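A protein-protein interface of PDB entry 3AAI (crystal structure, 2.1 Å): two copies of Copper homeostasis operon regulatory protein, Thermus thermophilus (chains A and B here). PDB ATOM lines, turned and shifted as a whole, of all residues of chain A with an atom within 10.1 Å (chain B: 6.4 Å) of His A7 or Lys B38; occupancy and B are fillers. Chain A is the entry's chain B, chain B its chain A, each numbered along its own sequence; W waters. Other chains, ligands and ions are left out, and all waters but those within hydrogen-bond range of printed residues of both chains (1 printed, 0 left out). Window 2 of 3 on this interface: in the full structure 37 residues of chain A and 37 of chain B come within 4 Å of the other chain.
His A7 touches just these residues of chain B: Glu B37 and Lys B38.
Lys B38 touches just these residues of chain A: Leu A6 and His A7.
Of the printed residues of chain A, Asp B36 touches Arg A13 (3.9 Å).
Of chain A, only Leu A6 (3.6 Å), His A7 (3.5 Å) and Leu A8 (3.7 Å) come within 4 Å of Glu B37.
Printed residues of chain B within 4 Å of Leu A8: Glu B37.
Of the printed residues of chain A, Leu B34 touches Arg A13 (2.9 Å).
Ala A65 touches none of the printed residues of chain B.
The nearest printed residue of chain B that does not touch His A5 is Lys B38 (4.7 Å).
The backbone carbonyl oxygen of Leu A6 sits at hydrogen-bond distance from the backbone NH of Val B39 (2.8 Å).
NZ of Lys B38 is in hydrogen-bond range of ND1 of His A7 (2.9 Å).
The backbone NH (N) of His A5 lies within hydrogen-bond range of the backbone carbonyl oxygen (O) of Val B39.
Printed residues of chain B that touch a printed residue of chain A: Leu B34, Asp B36, Glu B37, Lys B38, Val B39 and Tyr B40.
Hydrophobic or aromatic side chains of chain B that line the printed part of chain A: Tyr B40.
Printed residues of chain A that touch a printed residue of chain B: His A5, Leu A6, His A7, Leu A8 and Arg A13.
No position is printed for both chains.
Of the 10 pairs that touch across the chains among the printed residues, none has its exchanged pair printed and touching as well.
OD2 of Asp B36 is in hydrogen-bond range of N of Lys B38 (2.9 Å).
Water W1 lies within hydrogen-bond range of O of Leu A8 (2.5 Å), NE of Arg A13 (2.8 Å) and O of Glu B37 (2.9 Å).
Among the printed residues, merely in contact across the chains: Arg A13 with Leu B34 (2.9 Å), His A5 with Tyr B40 (3.2 Å), His A7 with Glu B37 (3.5 Å), Leu A6 with Glu B37 (3.6 Å), Leu A6 with Lys B38 (3.6 Å), Leu A8 with Glu B37 (3.7 Å) and Arg A13 with Asp B36 (3.9 Å).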
ATOM      1  N   HIS A   5      30.485   3.653  -0.013  1.00  0.00           N
ATOM      2  CA  HIS A   5      29.871   3.535   1.340  1.00  0.00           C
ATOM      3  C   HIS A   5      28.367   3.804   1.254  1.00  0.00           C
ATOM      4  O   HIS A   5      27.590   3.334   2.088  1.00  0.00           O
ATOM      5  CB  HIS A   5      30.524   4.535   2.296  1.00  0.00           C
ATOM      6  CG  HIS A   5      30.386   4.170   3.739  1.00  0.00           C
ATOM      7  ND1 HIS A   5      30.898   3.001   4.262  1.00  0.00           N
ATOM      8  CD2 HIS A   5      29.799   4.820   4.773  1.00  0.00           C
ATOM      9  CE1 HIS A   5      30.632   2.947   5.555  1.00  0.00           C
ATOM     10  NE2 HIS A   5      29.966   4.038   5.890  1.00  0.00           N
ATOM     11  N   LEU A   6      27.963   4.561   0.239  1.00  0.00           N
ATOM     12  CA  LEU A   6      26.559   4.883   0.035  1.00  0.00           C
ATOM     13  C   LEU A   6      26.179   4.912  -1.445  1.00  0.00           C
ATOM     14  O   LEU A   6      26.887   5.494  -2.275  1.00  0.00           O
ATOM     15  CB  LEU A   6      26.223   6.239   0.658  1.00  0.00           C
ATOM     16  CG  LEU A   6      24.776   6.695   0.439  1.00  0.00           C
ATOM     17  CD1 LEU A   6      23.839   5.696   1.107  1.00  0.00           C
ATOM     18  CD2 LEU A   6      24.567   8.095   1.008  1.00  0.00           C
ATOM     19  N   HIS A   7      25.053   4.282  -1.769  1.00  0.00           N
ATOM     20  CA  HIS A   7      24.569   4.258  -3.141  1.00  0.00           C
ATOM     21  C   HIS A   7      23.673   5.476  -3.327  1.00  0.00           C
ATOM     22  O   HIS A   7      22.448   5.383  -3.282  1.00  0.00           O
ATOM     23  CB  HIS A   7      23.789   2.971  -3.412  1.00  0.00           C
ATOM     24  CG  HIS A   7      23.448   2.770  -4.854  1.00  0.00           C
ATOM     25  ND1 HIS A   7      23.198   1.525  -5.391  1.00  0.00           N
ATOM     26  CD2 HIS A   7      23.329   3.651  -5.875  1.00  0.00           C
ATOM     27  CE1 HIS A   7      22.945   1.650  -6.682  1.00  0.00           C
ATOM     28  NE2 HIS A   7      23.018   2.929  -7.000  1.00  0.00           N
ATOM     29  N   LEU A   8      24.314   6.620  -3.528  1.00  0.00           N
ATOM     30  CA  LEU A   8      23.639   7.898  -3.705  1.00  0.00           C
ATOM     31  C   LEU A   8      22.523   7.856  -4.752  1.00  0.00           C
ATOM     32  O   LEU A   8      22.657   7.223  -5.796  1.00  0.00           O
ATOM     33  CB  LEU A   8      24.679   8.950  -4.088  1.00  0.00           C
ATOM     34  CG  LEU A   8      24.358  10.438  -3.959  1.00  0.00           C
ATOM     35  CD1 LEU A   8      23.975  10.770  -2.526  1.00  0.00           C
ATOM     36  CD2 LEU A   8      25.583  11.238  -4.375  1.00  0.00           C
ATOM     37  N   ASP A   9      21.418   8.536  -4.455  1.00  0.00           N
ATOM     38  CA  ASP A   9      20.275   8.609  -5.359  1.00  0.00           C
ATOM     39  C   ASP A   9      20.728   9.198  -6.699  1.00  0.00           C
ATOM     40  O   ASP A   9      21.233  10.316  -6.745  1.00  0.00           O
ATOM     41  CB  ASP A   9      19.197   9.515  -4.755  1.00  0.00           C
ATOM     42  CG  ASP A   9      17.909   9.537  -5.575  1.00  0.00           C
ATOM     43  OD1 ASP A   9      17.953   9.290  -6.803  1.00  0.00           O
ATOM     44  OD2 ASP A   9      16.845   9.821  -4.983  1.00  0.00           O
ATOM     45  N   PRO A  10      20.546   8.457  -7.805  1.00  0.00           N
ATOM     46  CA  PRO A  10      20.947   8.943  -9.132  1.00  0.00           C
ATOM     47  C   PRO A  10      20.527  10.403  -9.337  1.00  0.00           C
ATOM     48  O   PRO A  10      21.233  11.191  -9.972  1.00  0.00           O
ATOM     49  CB  PRO A  10      20.225   7.987 -10.075  1.00  0.00           C
ATOM     50  CG  PRO A  10      20.264   6.693  -9.309  1.00  0.00           C
ATOM     51  CD  PRO A  10      19.901   7.134  -7.903  1.00  0.00           C
ATOM     52  N   LYS A  11      19.369  10.745  -8.779  1.00  0.00           N
ATOM     53  CA  LYS A  11      18.816  12.093  -8.851  1.00  0.00           C
ATOM     54  C   LYS A  11      19.793  13.111  -8.250  1.00  0.00           C
ATOM     55  O   LYS A  11      20.098  14.139  -8.865  1.00  0.00           O
ATOM     56  CB  LYS A  11      17.487  12.127  -8.090  1.00  0.00           C
ATOM     57  CG  LYS A  11      16.911  13.507  -7.835  1.00  0.00           C
ATOM     58  CD  LYS A  11      15.716  13.402  -6.893  1.00  0.00           C
ATOM     59  CE  LYS A  11      15.175  14.767  -6.500  1.00  0.00           C
ATOM     60  NZ  LYS A  11      14.052  14.649  -5.521  1.00  0.00           N
ATOM     61  N   VAL A  12      20.278  12.818  -7.049  1.00  0.00           N
ATOM     62  CA  VAL A  12      21.216  13.701  -6.365  1.00  0.00           C
ATOM     63  C   VAL A  12      22.560  13.666  -7.079  1.00  0.00           C
ATOM     64  O   VAL A  12      23.189  14.701  -7.307  1.00  0.00           O
ATOM     65  CB  VAL A  12      21.417  13.266  -4.899  1.00  0.00           C
ATOM     66  CG1 VAL A  12      22.462  14.152  -4.222  1.00  0.00           C
ATOM     67  CG2 VAL A  12      20.094  13.351  -4.156  1.00  0.00           C
ATOM     68  N   ARG A  13      22.983  12.457  -7.425  1.00  0.00           N
ATOM     69  CA  ARG A  13      24.242  12.231  -8.114  1.00  0.00           C
ATOM     70  C   ARG A  13      24.322  13.049  -9.396  1.00  0.00           C
ATOM     71  O   ARG A  13      25.282  13.788  -9.606  1.00  0.00           O
ATOM     72  CB  ARG A  13      24.393  10.734  -8.420  1.00  0.00           C
ATOM     73  CG  ARG A  13      25.552  10.380  -9.328  1.00  0.00           C
ATOM     74  CD  ARG A  13      25.899   8.894  -9.248  1.00  0.00           C
ATOM     75  NE  ARG A  13      24.808   8.008  -9.646  1.00  0.00           N
ATOM     76  CZ  ARG A  13      24.233   8.017 -10.845  1.00  0.00           C
ATOM     77  NH1 ARG A  13      24.638   8.875 -11.772  1.00  0.00           N
ATOM     78  NH2 ARG A  13      23.267   7.155 -11.125  1.00  0.00           N
ATOM     79  N   ALA A  65      22.529  14.214   2.045  1.00  0.00           N
ATOM     80  CA  ALA A  65      22.400  12.788   1.744  1.00  0.00           C
ATOM     81  C   ALA A  65      23.099  11.937   2.794  1.00  0.00           C
ATOM     82  O   ALA A  65      22.602  10.875   3.178  1.00  0.00           O
ATOM     83  CB  ALA A  65      22.976  12.481   0.366  1.00  0.00           C
ATOM     84  N   HIS A  66      24.262  12.399   3.243  1.00  0.00           N
ATOM     85  CA  HIS A  66      25.013  11.683   4.261  1.00  0.00           C
ATOM     86  C   HIS A  66      24.214  11.653   5.561  1.00  0.00           C
ATOM     87  O   HIS A  66      24.083  10.606   6.189  1.00  0.00           O
ATOM     88  CB  HIS A  66      26.354  12.371   4.515  1.00  0.00           C
ATOM     89  CG  HIS A  66      27.204  11.678   5.532  1.00  0.00           C
ATOM     90  ND1 HIS A  66      27.829  10.476   5.285  1.00  0.00           N
ATOM     91  CD2 HIS A  66      27.526  12.015   6.803  1.00  0.00           C
ATOM     92  CE1 HIS A  66      28.503  10.102   6.360  1.00  0.00           C
ATOM     93  NE2 HIS A  66      28.335  11.020   7.295  1.00  0.00           N
ATOM     94  N   ASP A  69      20.999   9.439   5.674  1.00  0.00           N
ATOM     95  CA  ASP A  69      21.420   8.051   5.808  1.00  0.00           C
ATOM     96  C   ASP A  69      21.699   7.677   7.260  1.00  0.00           C
ATOM     97  O   ASP A  69      21.003   6.840   7.833  1.00  0.00           O
ATOM     98  CB  ASP A  69      22.673   7.800   4.963  1.00  0.00           C
ATOM     99  CG  ASP A  69      23.336   6.475   5.282  1.00  0.00           C
ATOM    100  OD1 ASP A  69      22.641   5.437   5.250  1.00  0.00           O
ATOM    101  OD2 ASP A  69      24.554   6.472   5.562  1.00  0.00           O
ATOM    102  N   HIS A  70      22.712   8.307   7.852  1.00  0.00           N
ATOM    103  CA  HIS A  70      23.105   8.031   9.234  1.00  0.00           C
ATOM    104  C   HIS A  70      22.089   8.394  10.320  1.00  0.00           C
ATOM    105  O   HIS A  70      22.184   7.916  11.454  1.00  0.00           O
ATOM    106  CB  HIS A  70      24.451   8.695   9.523  1.00  0.00           C
ATOM    107  CG  HIS A  70      25.605   8.003   8.867  1.00  0.00           C
ATOM    108  ND1 HIS A  70      26.262   6.939   9.447  1.00  0.00           N
ATOM    109  CD2 HIS A  70      26.172   8.177   7.650  1.00  0.00           C
ATOM    110  CE1 HIS A  70      27.184   6.487   8.615  1.00  0.00           C
ATOM    111  NE2 HIS A  70      27.149   7.221   7.517  1.00  0.00           N
ATOM    112  N   MET B  33      34.418  10.646  -8.822  1.00  0.00           N
ATOM    113  CA  MET B  33      33.927  10.011  -7.604  1.00  0.00           C
ATOM    114  C   MET B  33      32.400   9.936  -7.626  1.00  0.00           C
ATOM    115  O   MET B  33      31.816   8.910  -7.285  1.00  0.00           O
ATOM    116  CB  MET B  33      34.370  10.804  -6.375  1.00  0.00           C
ATOM    117  CG  MET B  33      35.869  10.762  -6.115  1.00  0.00           C
ATOM    118  SD  MET B  33      36.389  11.934  -4.673  1.00  0.00           S
ATOM    119  CE  MET B  33      35.966  10.776  -3.176  1.00  0.00           C
ATOM    120  N   LEU B  34      31.762  11.031  -8.023  1.00  0.00           N
ATOM    121  CA  LEU B  34      30.309  11.081  -8.086  1.00  0.00           C
ATOM    122  C   LEU B  34      29.743  10.248  -9.226  1.00  0.00           C
ATOM    123  O   LEU B  34      28.655   9.692  -9.104  1.00  0.00           O
ATOM    124  CB  LEU B  34      29.831  12.532  -8.207  1.00  0.00           C
ATOM    125  CG  LEU B  34      29.988  13.330  -6.908  1.00  0.00           C
ATOM    126  CD1 LEU B  34      29.716  14.793  -7.155  1.00  0.00           C
ATOM    127  CD2 LEU B  34      29.040  12.775  -5.860  1.00  0.00           C
ATOM    128  N   ASP B  36      30.425   7.595  -9.883  1.00  0.00           N
ATOM    129  CA  ASP B  36      30.495   6.227  -9.404  1.00  0.00           C
ATOM    130  C   ASP B  36      29.223   6.007  -8.594  1.00  0.00           C
ATOM    131  O   ASP B  36      28.859   6.835  -7.761  1.00  0.00           O
ATOM    132  CB  ASP B  36      31.728   6.036  -8.520  1.00  0.00           C
ATOM    133  CG  ASP B  36      31.810   4.644  -7.923  1.00  0.00           C
ATOM    134  OD1 ASP B  36      32.816   4.352  -7.242  1.00  0.00           O
ATOM    135  OD2 ASP B  36      30.870   3.844  -8.129  1.00  0.00           O
ATOM    136  N   GLU B  37      28.538   4.900  -8.849  1.00  0.00           N
ATOM    137  CA  GLU B  37      27.303   4.601  -8.145  1.00  0.00           C
ATOM    138  C   GLU B  37      27.513   4.550  -6.634  1.00  0.00           C
ATOM    139  O   GLU B  37      26.669   5.010  -5.865  1.00  0.00           O
ATOM    140  CB  GLU B  37      26.724   3.284  -8.666  1.00  0.00           C
ATOM    141  CG  GLU B  37      26.438   3.326 -10.167  1.00  0.00           C
ATOM    142  CD  GLU B  37      25.761   2.074 -10.686  1.00  0.00           C
ATOM    143  OE1 GLU B  37      25.452   2.026 -11.898  1.00  0.00           O
ATOM    144  OE2 GLU B  37      25.534   1.142  -9.889  1.00  0.00           O
ATOM    145  N   LYS B  38      28.649   4.006  -6.213  1.00  0.00           N
ATOM    146  CA  LYS B  38      28.974   3.912  -4.794  1.00  0.00           C
ATOM    147  C   LYS B  38      29.849   5.111  -4.439  1.00  0.00           C
ATOM    148  O   LYS B  38      30.890   5.327  -5.058  1.00  0.00           O
ATOM    149  CB  LYS B  38      29.716   2.605  -4.517  1.00  0.00           C
ATOM    150  CG  LYS B  38      29.004   1.380  -5.074  1.00  0.00           C
ATOM    151  CD  LYS B  38      27.591   1.267  -4.517  1.00  0.00           C
ATOM    152  CE  LYS B  38      26.836   0.101  -5.137  1.00  0.00           C
ATOM    153  NZ  LYS B  38      25.501  -0.083  -4.503  1.00  0.00           N
ATOM    154  N   VAL B  39      29.425   5.887  -3.445  1.00  0.00           N
ATOM    155  CA  VAL B  39      30.165   7.079  -3.045  1.00  0.00           C
ATOM    156  C   VAL B  39      30.425   7.219  -1.546  1.00  0.00           C
ATOM    157  O   VAL B  39      29.564   6.924  -0.716  1.00  0.00           O
ATOM    158  CB  VAL B  39      29.425   8.356  -3.511  1.00  0.00           C
ATOM    159  CG1 VAL B  39      30.221   9.597  -3.125  1.00  0.00           C
ATOM    160  CG2 VAL B  39      29.200   8.303  -5.012  1.00  0.00           C
ATOM    161  N   TYR B  40      31.624   7.684  -1.214  1.00  0.00           N
ATOM    162  CA  TYR B  40      32.023   7.909   0.172  1.00  0.00           C
ATOM    163  C   TYR B  40      31.778   9.386   0.487  1.00  0.00           C
ATOM    164  O   TYR B  40      32.662  10.224   0.308  1.00  0.00           O
ATOM    165  CB  TYR B  40      33.505   7.565   0.346  1.00  0.00           C
ATOM    166  CG  TYR B  40      33.788   6.081   0.265  1.00  0.00           C
ATOM    167  CD1 TYR B  40      33.527   5.245   1.351  1.00  0.00           C
ATOM    168  CD2 TYR B  40      34.279   5.505  -0.907  1.00  0.00           C
ATOM    169  CE1 TYR B  40      33.742   3.873   1.272  1.00  0.00           C
ATOM    170  CE2 TYR B  40      34.498   4.130  -0.996  1.00  0.00           C
ATOM    171  CZ  TYR B  40      34.227   3.322   0.099  1.00  0.00           C
ATOM    172  OH  TYR B  40      34.435   1.964   0.024  1.00  0.00           O
HETATM  173  O   HOH W   1      24.642   6.622  -7.204  1.00  0.00           O
